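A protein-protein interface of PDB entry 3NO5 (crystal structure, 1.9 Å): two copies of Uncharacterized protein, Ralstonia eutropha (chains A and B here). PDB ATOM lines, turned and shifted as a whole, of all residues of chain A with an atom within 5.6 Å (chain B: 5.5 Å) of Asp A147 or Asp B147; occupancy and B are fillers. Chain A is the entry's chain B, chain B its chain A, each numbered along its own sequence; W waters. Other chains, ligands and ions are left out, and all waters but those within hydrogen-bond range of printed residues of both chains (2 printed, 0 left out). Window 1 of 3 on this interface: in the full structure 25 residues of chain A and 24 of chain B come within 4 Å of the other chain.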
ATOM      1  N   SER A 112     -29.414 -20.949 -21.644  1.00  0.00           N
ATOM      2  CA  SER A 112     -29.938 -20.278 -22.834  1.00  0.00           C
ATOM      3  C   SER A 112     -28.842 -20.121 -23.880  1.00  0.00           C
ATOM      4  O   SER A 112     -27.662 -20.027 -23.533  1.00  0.00           O
ATOM      5  CB  SER A 112     -30.525 -18.921 -22.474  1.00  0.00           C
ATOM      6  OG  SER A 112     -31.639 -19.066 -21.610  1.00  0.00           O
ATOM      7  N   VAL A 113     -29.224 -20.153 -25.159  1.00  0.00           N
ATOM      8  CA  VAL A 113     -28.284 -20.058 -26.276  1.00  0.00           C
ATOM      9  C   VAL A 113     -28.988 -19.407 -27.475  1.00  0.00           C
ATOM     10  O   VAL A 113     -30.214 -19.488 -27.587  1.00  0.00           O
ATOM     11  CB  VAL A 113     -27.704 -21.470 -26.640  1.00  0.00           C
ATOM     12  CG1 VAL A 113     -28.769 -22.366 -27.276  1.00  0.00           C
ATOM     13  CG2 VAL A 113     -26.479 -21.355 -27.543  1.00  0.00           C
ATOM     14  N   ALA A 145     -26.817 -29.933 -23.947  1.00  0.00           N
ATOM     15  CA  ALA A 145     -25.732 -28.968 -23.835  1.00  0.00           C
ATOM     16  C   ALA A 145     -25.460 -28.306 -25.176  1.00  0.00           C
ATOM     17  O   ALA A 145     -24.780 -28.884 -26.033  1.00  0.00           O
ATOM     18  CB  ALA A 145     -24.474 -29.644 -23.309  1.00  0.00           C
ATOM     19  N   PHE A 146     -26.041 -27.109 -25.382  1.00  0.00           N
ATOM     20  CA  PHE A 146     -25.859 -26.334 -26.612  1.00  0.00           C
ATOM     21  C   PHE A 146     -24.638 -25.419 -26.499  1.00  0.00           C
ATOM     22  O   PHE A 146     -24.254 -24.783 -27.477  1.00  0.00           O
ATOM     23  CB  PHE A 146     -27.110 -25.502 -26.918  1.00  0.00           C
ATOM     24  CG  PHE A 146     -28.345 -26.310 -27.230  1.00  0.00           C
ATOM     25  CD1 PHE A 146     -28.631 -26.699 -28.535  1.00  0.00           C
ATOM     26  CD2 PHE A 146     -29.255 -26.636 -26.229  1.00  0.00           C
ATOM     27  CE1 PHE A 146     -29.792 -27.421 -28.829  1.00  0.00           C
ATOM     28  CE2 PHE A 146     -30.425 -27.344 -26.528  1.00  0.00           C
ATOM     29  CZ  PHE A 146     -30.680 -27.741 -27.822  1.00  0.00           C
ATOM     30  N   ASP A 147     -24.053 -25.328 -25.289  1.00  0.00           N
ATOM     31  CA  ASP A 147     -22.875 -24.507 -25.025  1.00  0.00           C
ATOM     32  C   ASP A 147     -22.137 -25.053 -23.794  1.00  0.00           C
ATOM     33  O   ASP A 147     -22.716 -25.819 -23.025  1.00  0.00           O
ATOM     34  CB  ASP A 147     -23.277 -23.032 -24.813  1.00  0.00           C
ATOM     35  CG  ASP A 147     -22.255 -22.029 -25.320  1.00  0.00           C
ATOM     36  OD1 ASP A 147     -21.077 -22.408 -25.478  1.00  0.00           O
ATOM     37  OD2 ASP A 147     -22.613 -20.853 -25.467  1.00  0.00           O
ATOM     38  N   LEU A 148     -20.863 -24.662 -23.616  1.00  0.00           N
ATOM     39  CA  LEU A 148     -19.998 -25.174 -22.545  1.00  0.00           C
ATOM     40  C   LEU A 148     -20.567 -25.012 -21.115  1.00  0.00           C
ATOM     41  O   LEU A 148     -20.506 -25.964 -20.328  1.00  0.00           O
ATOM     42  CB  LEU A 148     -18.591 -24.552 -22.649  1.00  0.00           C
ATOM     43  CG  LEU A 148     -17.517 -25.087 -21.672  1.00  0.00           C
ATOM     44  CD1 LEU A 148     -17.311 -26.594 -21.837  1.00  0.00           C
ATOM     45  CD2 LEU A 148     -16.215 -24.369 -21.870  1.00  0.00           C
ATOM     46  N   SER A 149     -21.106 -23.813 -20.775  1.00  0.00           N
ATOM     47  CA  SER A 149     -21.616 -23.541 -19.409  1.00  0.00           C
ATOM     48  C   SER A 149     -22.731 -24.503 -18.984  1.00  0.00           C
ATOM     49  O   SER A 149     -22.924 -24.726 -17.788  1.00  0.00           O
ATOM     50  CB  SER A 149     -22.097 -22.098 -19.282  1.00  0.00           C
ATOM     51  OG  SER A 149     -23.324 -21.898 -19.965  1.00  0.00           O
ATOM     52  N   MET A 150     -23.465 -25.071 -19.962  1.00  0.00           N
ATOM     53  CA  MET A 150     -24.564 -26.002 -19.681  1.00  0.00           C
ATOM     54  C   MET A 150     -24.068 -27.321 -19.081  1.00  0.00           C
ATOM     55  O   MET A 150     -24.803 -27.968 -18.337  1.00  0.00           O
ATOM     56  CB  MET A 150     -25.413 -26.236 -20.929  1.00  0.00           C
ATOM     57  CG  MET A 150     -26.033 -24.952 -21.467  1.00  0.00           C
ATOM     58  SD  MET A 150     -27.429 -25.236 -22.785  1.00  0.00           S
ATOM     59  CE  MET A 150     -27.391 -23.526 -23.595  1.00  0.00           C
ATOM     60  N   ILE A 151     -22.802 -27.691 -19.357  1.00  0.00           N
ATOM     61  CA  ILE A 151     -22.190 -28.875 -18.744  1.00  0.00           C
ATOM     62  C   ILE A 151     -21.932 -28.587 -17.261  1.00  0.00           C
ATOM     63  O   ILE A 151     -22.266 -29.410 -16.405  1.00  0.00           O
ATOM     64  CB  ILE A 151     -20.884 -29.288 -19.488  1.00  0.00           C
ATOM     65  CG1 ILE A 151     -21.148 -29.507 -20.998  1.00  0.00           C
ATOM     66  CG2 ILE A 151     -20.240 -30.544 -18.831  1.00  0.00           C
ATOM     67  CD1 ILE A 151     -19.900 -29.629 -21.833  1.00  0.00           C
ATOM     68  N   MET A 179     -23.351 -23.519 -31.000  1.00  0.00           N
ATOM     69  CA  MET A 179     -22.012 -24.118 -31.076  1.00  0.00           C
ATOM     70  C   MET A 179     -21.793 -24.775 -32.442  1.00  0.00           C
ATOM     71  O   MET A 179     -22.519 -25.704 -32.800  1.00  0.00           O
ATOM     72  CB  MET A 179     -21.806 -25.142 -29.942  1.00  0.00           C
ATOM     73  CG  MET A 179     -20.388 -25.748 -29.905  1.00  0.00           C
ATOM     74  SD  MET A 179     -18.997 -24.428 -29.565  1.00  0.00           S
ATOM     75  CE  MET A 179     -19.472 -23.920 -27.792  1.00  0.00           C
ATOM     76  N   TYR A 189     -15.325 -30.987 -24.276  1.00  0.00           N
ATOM     77  CA  TYR A 189     -16.626 -31.312 -23.664  1.00  0.00           C
ATOM     78  C   TYR A 189     -16.513 -32.625 -22.867  1.00  0.00           C
ATOM     79  O   TYR A 189     -16.934 -32.687 -21.711  1.00  0.00           O
ATOM     80  CB  TYR A 189     -17.704 -31.486 -24.764  1.00  0.00           C
ATOM     81  CG  TYR A 189     -18.400 -30.214 -25.223  1.00  0.00           C
ATOM     82  CD1 TYR A 189     -18.066 -28.975 -24.684  1.00  0.00           C
ATOM     83  CD2 TYR A 189     -19.420 -30.259 -26.170  1.00  0.00           C
ATOM     84  CE1 TYR A 189     -18.750 -27.815 -25.056  1.00  0.00           C
ATOM     85  CE2 TYR A 189     -20.104 -29.108 -26.554  1.00  0.00           C
ATOM     86  CZ  TYR A 189     -19.764 -27.887 -25.999  1.00  0.00           C
ATOM     87  OH  TYR A 189     -20.442 -26.754 -26.380  1.00  0.00           O
ATOM     88  N   SER B 112     -26.368 -15.189 -26.105  1.00  0.00           N
ATOM     89  CA  SER B 112     -27.218 -15.128 -24.925  1.00  0.00           C
ATOM     90  C   SER B 112     -26.738 -16.126 -23.881  1.00  0.00           C
ATOM     91  O   SER B 112     -26.151 -17.154 -24.229  1.00  0.00           O
ATOM     92  CB  SER B 112     -28.670 -15.400 -25.294  1.00  0.00           C
ATOM     93  OG  SER B 112     -29.166 -14.387 -26.153  1.00  0.00           O
ATOM     94  N   VAL B 113     -26.943 -15.803 -22.603  1.00  0.00           N
ATOM     95  CA  VAL B 113     -26.506 -16.641 -21.481  1.00  0.00           C
ATOM     96  C   VAL B 113     -27.440 -16.430 -20.286  1.00  0.00           C
ATOM     97  O   VAL B 113     -28.057 -15.369 -20.174  1.00  0.00           O
ATOM     98  CB  VAL B 113     -25.017 -16.344 -21.109  1.00  0.00           C
ATOM     99  CG1 VAL B 113     -24.870 -14.961 -20.468  1.00  0.00           C
ATOM    100  CG2 VAL B 113     -24.435 -17.435 -20.206  1.00  0.00           C
ATOM    101  N   ALA B 145     -17.496 -12.348 -23.790  1.00  0.00           N
ATOM    102  CA  ALA B 145     -17.694 -13.785 -23.915  1.00  0.00           C
ATOM    103  C   ALA B 145     -18.105 -14.395 -22.583  1.00  0.00           C
ATOM    104  O   ALA B 145     -17.257 -14.640 -21.717  1.00  0.00           O
ATOM    105  CB  ALA B 145     -16.432 -14.449 -24.443  1.00  0.00           C
ATOM    106  N   PHE B 146     -19.422 -14.579 -22.390  1.00  0.00           N
ATOM    107  CA  PHE B 146     -19.975 -15.161 -21.163  1.00  0.00           C
ATOM    108  C   PHE B 146     -20.047 -16.690 -21.265  1.00  0.00           C
ATOM    109  O   PHE B 146     -20.364 -17.364 -20.281  1.00  0.00           O
ATOM    110  CB  PHE B 146     -21.367 -14.584 -20.874  1.00  0.00           C
ATOM    111  CG  PHE B 146     -21.389 -13.112 -20.541  1.00  0.00           C
ATOM    112  CD1 PHE B 146     -21.584 -12.159 -21.535  1.00  0.00           C
ATOM    113  CD2 PHE B 146     -21.276 -12.680 -19.228  1.00  0.00           C
ATOM    114  CE1 PHE B 146     -21.643 -10.800 -21.220  1.00  0.00           C
ATOM    115  CE2 PHE B 146     -21.326 -11.318 -18.916  1.00  0.00           C
ATOM    116  CZ  PHE B 146     -21.499 -10.387 -19.917  1.00  0.00           C
ATOM    117  N   ASP B 147     -19.777 -17.229 -22.466  1.00  0.00           N
ATOM    118  CA  ASP B 147     -19.796 -18.664 -22.728  1.00  0.00           C
ATOM    119  C   ASP B 147     -18.931 -18.970 -23.954  1.00  0.00           C
ATOM    120  O   ASP B 147     -18.611 -18.059 -24.725  1.00  0.00           O
ATOM    121  CB  ASP B 147     -21.244 -19.158 -22.942  1.00  0.00           C
ATOM    122  CG  ASP B 147     -21.508 -20.561 -22.419  1.00  0.00           C
ATOM    123  OD1 ASP B 147     -20.536 -21.336 -22.279  1.00  0.00           O
ATOM    124  OD2 ASP B 147     -22.685 -20.914 -22.248  1.00  0.00           O
ATOM    125  N   LEU B 148     -18.549 -20.249 -24.135  1.00  0.00           N
ATOM    126  CA  LEU B 148     -17.635 -20.681 -25.204  1.00  0.00           C
ATOM    127  C   LEU B 148     -18.082 -20.290 -26.632  1.00  0.00           C
ATOM    128  O   LEU B 148     -17.260 -19.793 -27.407  1.00  0.00           O
ATOM    129  CB  LEU B 148     -17.369 -22.199 -25.107  1.00  0.00           C
ATOM    130  CG  LEU B 148     -16.326 -22.776 -26.082  1.00  0.00           C
ATOM    131  CD1 LEU B 148     -14.962 -22.106 -25.902  1.00  0.00           C
ATOM    132  CD2 LEU B 148     -16.204 -24.276 -25.919  1.00  0.00           C
ATOM    133  N   SER B 149     -19.379 -20.505 -26.974  1.00  0.00           N
ATOM    134  CA  SER B 149     -19.892 -20.229 -28.334  1.00  0.00           C
ATOM    135  C   SER B 149     -19.715 -18.771 -28.761  1.00  0.00           C
ATOM    136  O   SER B 149     -19.622 -18.491 -29.955  1.00  0.00           O
ATOM    137  CB  SER B 149     -21.357 -20.639 -28.457  1.00  0.00           C
ATOM    138  OG  SER B 149     -22.209 -19.737 -27.770  1.00  0.00           O
ATOM    139  N   MET B 150     -19.648 -17.845 -27.784  1.00  0.00           N
ATOM    140  CA  MET B 150     -19.492 -16.418 -28.065  1.00  0.00           C
ATOM    141  C   MET B 150     -18.121 -16.083 -28.658  1.00  0.00           C
ATOM    142  O   MET B 150     -17.999 -15.103 -29.392  1.00  0.00           O
ATOM    143  CB  MET B 150     -19.778 -15.581 -26.816  1.00  0.00           C
ATOM    144  CG  MET B 150     -21.179 -15.786 -26.288  1.00  0.00           C
ATOM    145  SD  MET B 150     -21.729 -14.452 -25.005  1.00  0.00           S
ATOM    146  CE  MET B 150     -23.122 -15.445 -24.167  1.00  0.00           C
ATOM    147  N   ILE B 151     -17.102 -16.918 -28.377  1.00  0.00           N
ATOM    148  CA  ILE B 151     -15.775 -16.766 -28.979  1.00  0.00           C
ATOM    149  C   ILE B 151     -15.862 -17.140 -30.457  1.00  0.00           C
ATOM    150  O   ILE B 151     -15.360 -16.405 -31.311  1.00  0.00           O
ATOM    151  CB  ILE B 151     -14.707 -17.623 -28.233  1.00  0.00           C
ATOM    152  CG1 ILE B 151     -14.677 -17.289 -26.723  1.00  0.00           C
ATOM    153  CG2 ILE B 151     -13.308 -17.450 -28.881  1.00  0.00           C
ATOM    154  CD1 ILE B 151     -13.882 -18.264 -25.886  1.00  0.00           C
ATOM    155  N   MET B 179     -20.917 -18.856 -16.765  1.00  0.00           N
ATOM    156  CA  MET B 179     -19.677 -19.625 -16.686  1.00  0.00           C
ATOM    157  C   MET B 179     -19.003 -19.426 -15.322  1.00  0.00           C
ATOM    158  O   MET B 179     -18.643 -18.296 -14.968  1.00  0.00           O
ATOM    159  CB  MET B 179     -18.716 -19.231 -17.824  1.00  0.00           C
ATOM    160  CG  MET B 179     -17.432 -20.069 -17.853  1.00  0.00           C
ATOM    161  SD  MET B 179     -17.759 -21.965 -18.196  1.00  0.00           S
ATOM    162  CE  MET B 179     -18.357 -21.839 -19.976  1.00  0.00           C
ATOM    163  N   TYR B 189     -10.212 -21.303 -23.444  1.00  0.00           N
ATOM    164  CA  TYR B 189     -10.677 -20.044 -24.047  1.00  0.00           C
ATOM    165  C   TYR B 189      -9.521 -19.392 -24.836  1.00  0.00           C
ATOM    166  O   TYR B 189      -9.701 -18.999 -25.992  1.00  0.00           O
ATOM    167  CB  TYR B 189     -11.138 -19.064 -22.942  1.00  0.00           C
ATOM    168  CG  TYR B 189     -12.579 -19.200 -22.488  1.00  0.00           C
ATOM    169  CD1 TYR B 189     -13.418 -20.169 -23.034  1.00  0.00           C
ATOM    170  CD2 TYR B 189     -13.115 -18.331 -21.544  1.00  0.00           C
ATOM    171  CE1 TYR B 189     -14.761 -20.253 -22.668  1.00  0.00           C
ATOM    172  CE2 TYR B 189     -14.456 -18.401 -21.173  1.00  0.00           C
ATOM    173  CZ  TYR B 189     -15.275 -19.367 -21.732  1.00  0.00           C
ATOM    174  OH  TYR B 189     -16.595 -19.430 -21.360  1.00  0.00           O
HETATM  175  O   HOH W   1     -25.252 -20.400 -22.565  1.00  0.00           O
HETATM  176  O   HOH W   2     -24.579 -19.159 -25.327  1.00  0.00           O
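The side-chain hydroxyl of Ser A149 is in hydrogen-bond range of the side-chain carboxylate of Asp B147.
OD2 of Asp A147 sits at hydrogen-bond distance from OG of Ser B149, 2.6 Å away.
The backbone carbonyl oxygen (O) of Ser A112 lies close to the backbone carbonyl oxygen (O) of Ser B112, 3.3 Å away.
OD2 of Asp A147 sits close to OD2 of Asp B147 (3.2 Å).
N of Leu B148 lies within hydrogen-bond range of OH of Tyr B189 (3.5 Å).
The backbone NH of Leu A148 is in hydrogen-bond range of the side-chain hydroxyl of Tyr A189 (3.5 Å).
Among the printed residues, pairs that only touch across the chains: Ser A149 with Met B179, Met A179 with Ser B149, Asp A147 with Leu B148, Leu A148 with Asp B147, Leu A148 with Leu B148, Met A179 with Leu B148 and Leu A148 with Met B179.
Of the printed residues of chain B, Ser A112 touches Ser B112 (3.3 Å).
Asp A147 touches just these residues of chain B: Asp B147, Leu B148 and Ser B149.
Printed residues of chain B within 4 Å of Met A179: Leu B148 and Ser B149.
Printed residues of chain A within 4 Å of Ser B112: Ser A112.
Asp B147 touches just these residues of chain A: Asp A147 (3.2 Å), Leu A148 (3.6 Å) and Ser A149 (2.6 Å).
Printed residues of chain A within 4 Å of Leu B148: Asp A147 (3.6 Å), Leu A148 (3.6 Å) and Met A179 (3.8 Å).
Printed residues of chain A within 4 Å of Ser B149: Asp A147 and Met A179.
The nearest printed residue of chain B that does not touch Ser A112 is Val B113 (4.1 Å).
Of the 11 printed residues of chain B, 5 touch a printed residue of chain A.
Printed residues of chain B that touch a printed residue of chain A: Ser B112, Asp B147, Leu B148, Ser B149 and Met B179.
Hydrophobic or aromatic side chains of chain B within 4 Å of the printed part of chain A: Leu B148 and Met B179.
Hydrophobic or aromatic side chains of chain A that line the printed part of chain B: Leu A148 and Met A179.
Among the printed residues, 11 pairs touch across the chains.
Asp A147 touches Leu B148, and with the chains exchanged Leu A148 touches Asp B147.
Asp A147 touches Ser B149, and with the chains exchanged Ser A149 touches Asp B147.
Leu B148 touches its own counterpart, Leu A148.
Ser A149 touches Met B179, and with the chains exchanged Met A179 touches Ser B149.
Positions printed for both chains: 112, 113, 145, 146, 147, 148, 149, 150, 151, 179 and 189.
Of the 11 pairs that touch across the chains among the printed residues, 11 have their exchanged pair printed and touching as well.
Water W2 lies within hydrogen-bond range of OD2 of Asp A147, O of Ser B112 and OG of Ser B149.
Water W1 bridges the backbone carbonyl oxygen of Ser A112 (2.6 Å) and the side-chain carboxylate of Asp B147 (2.6 Å).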
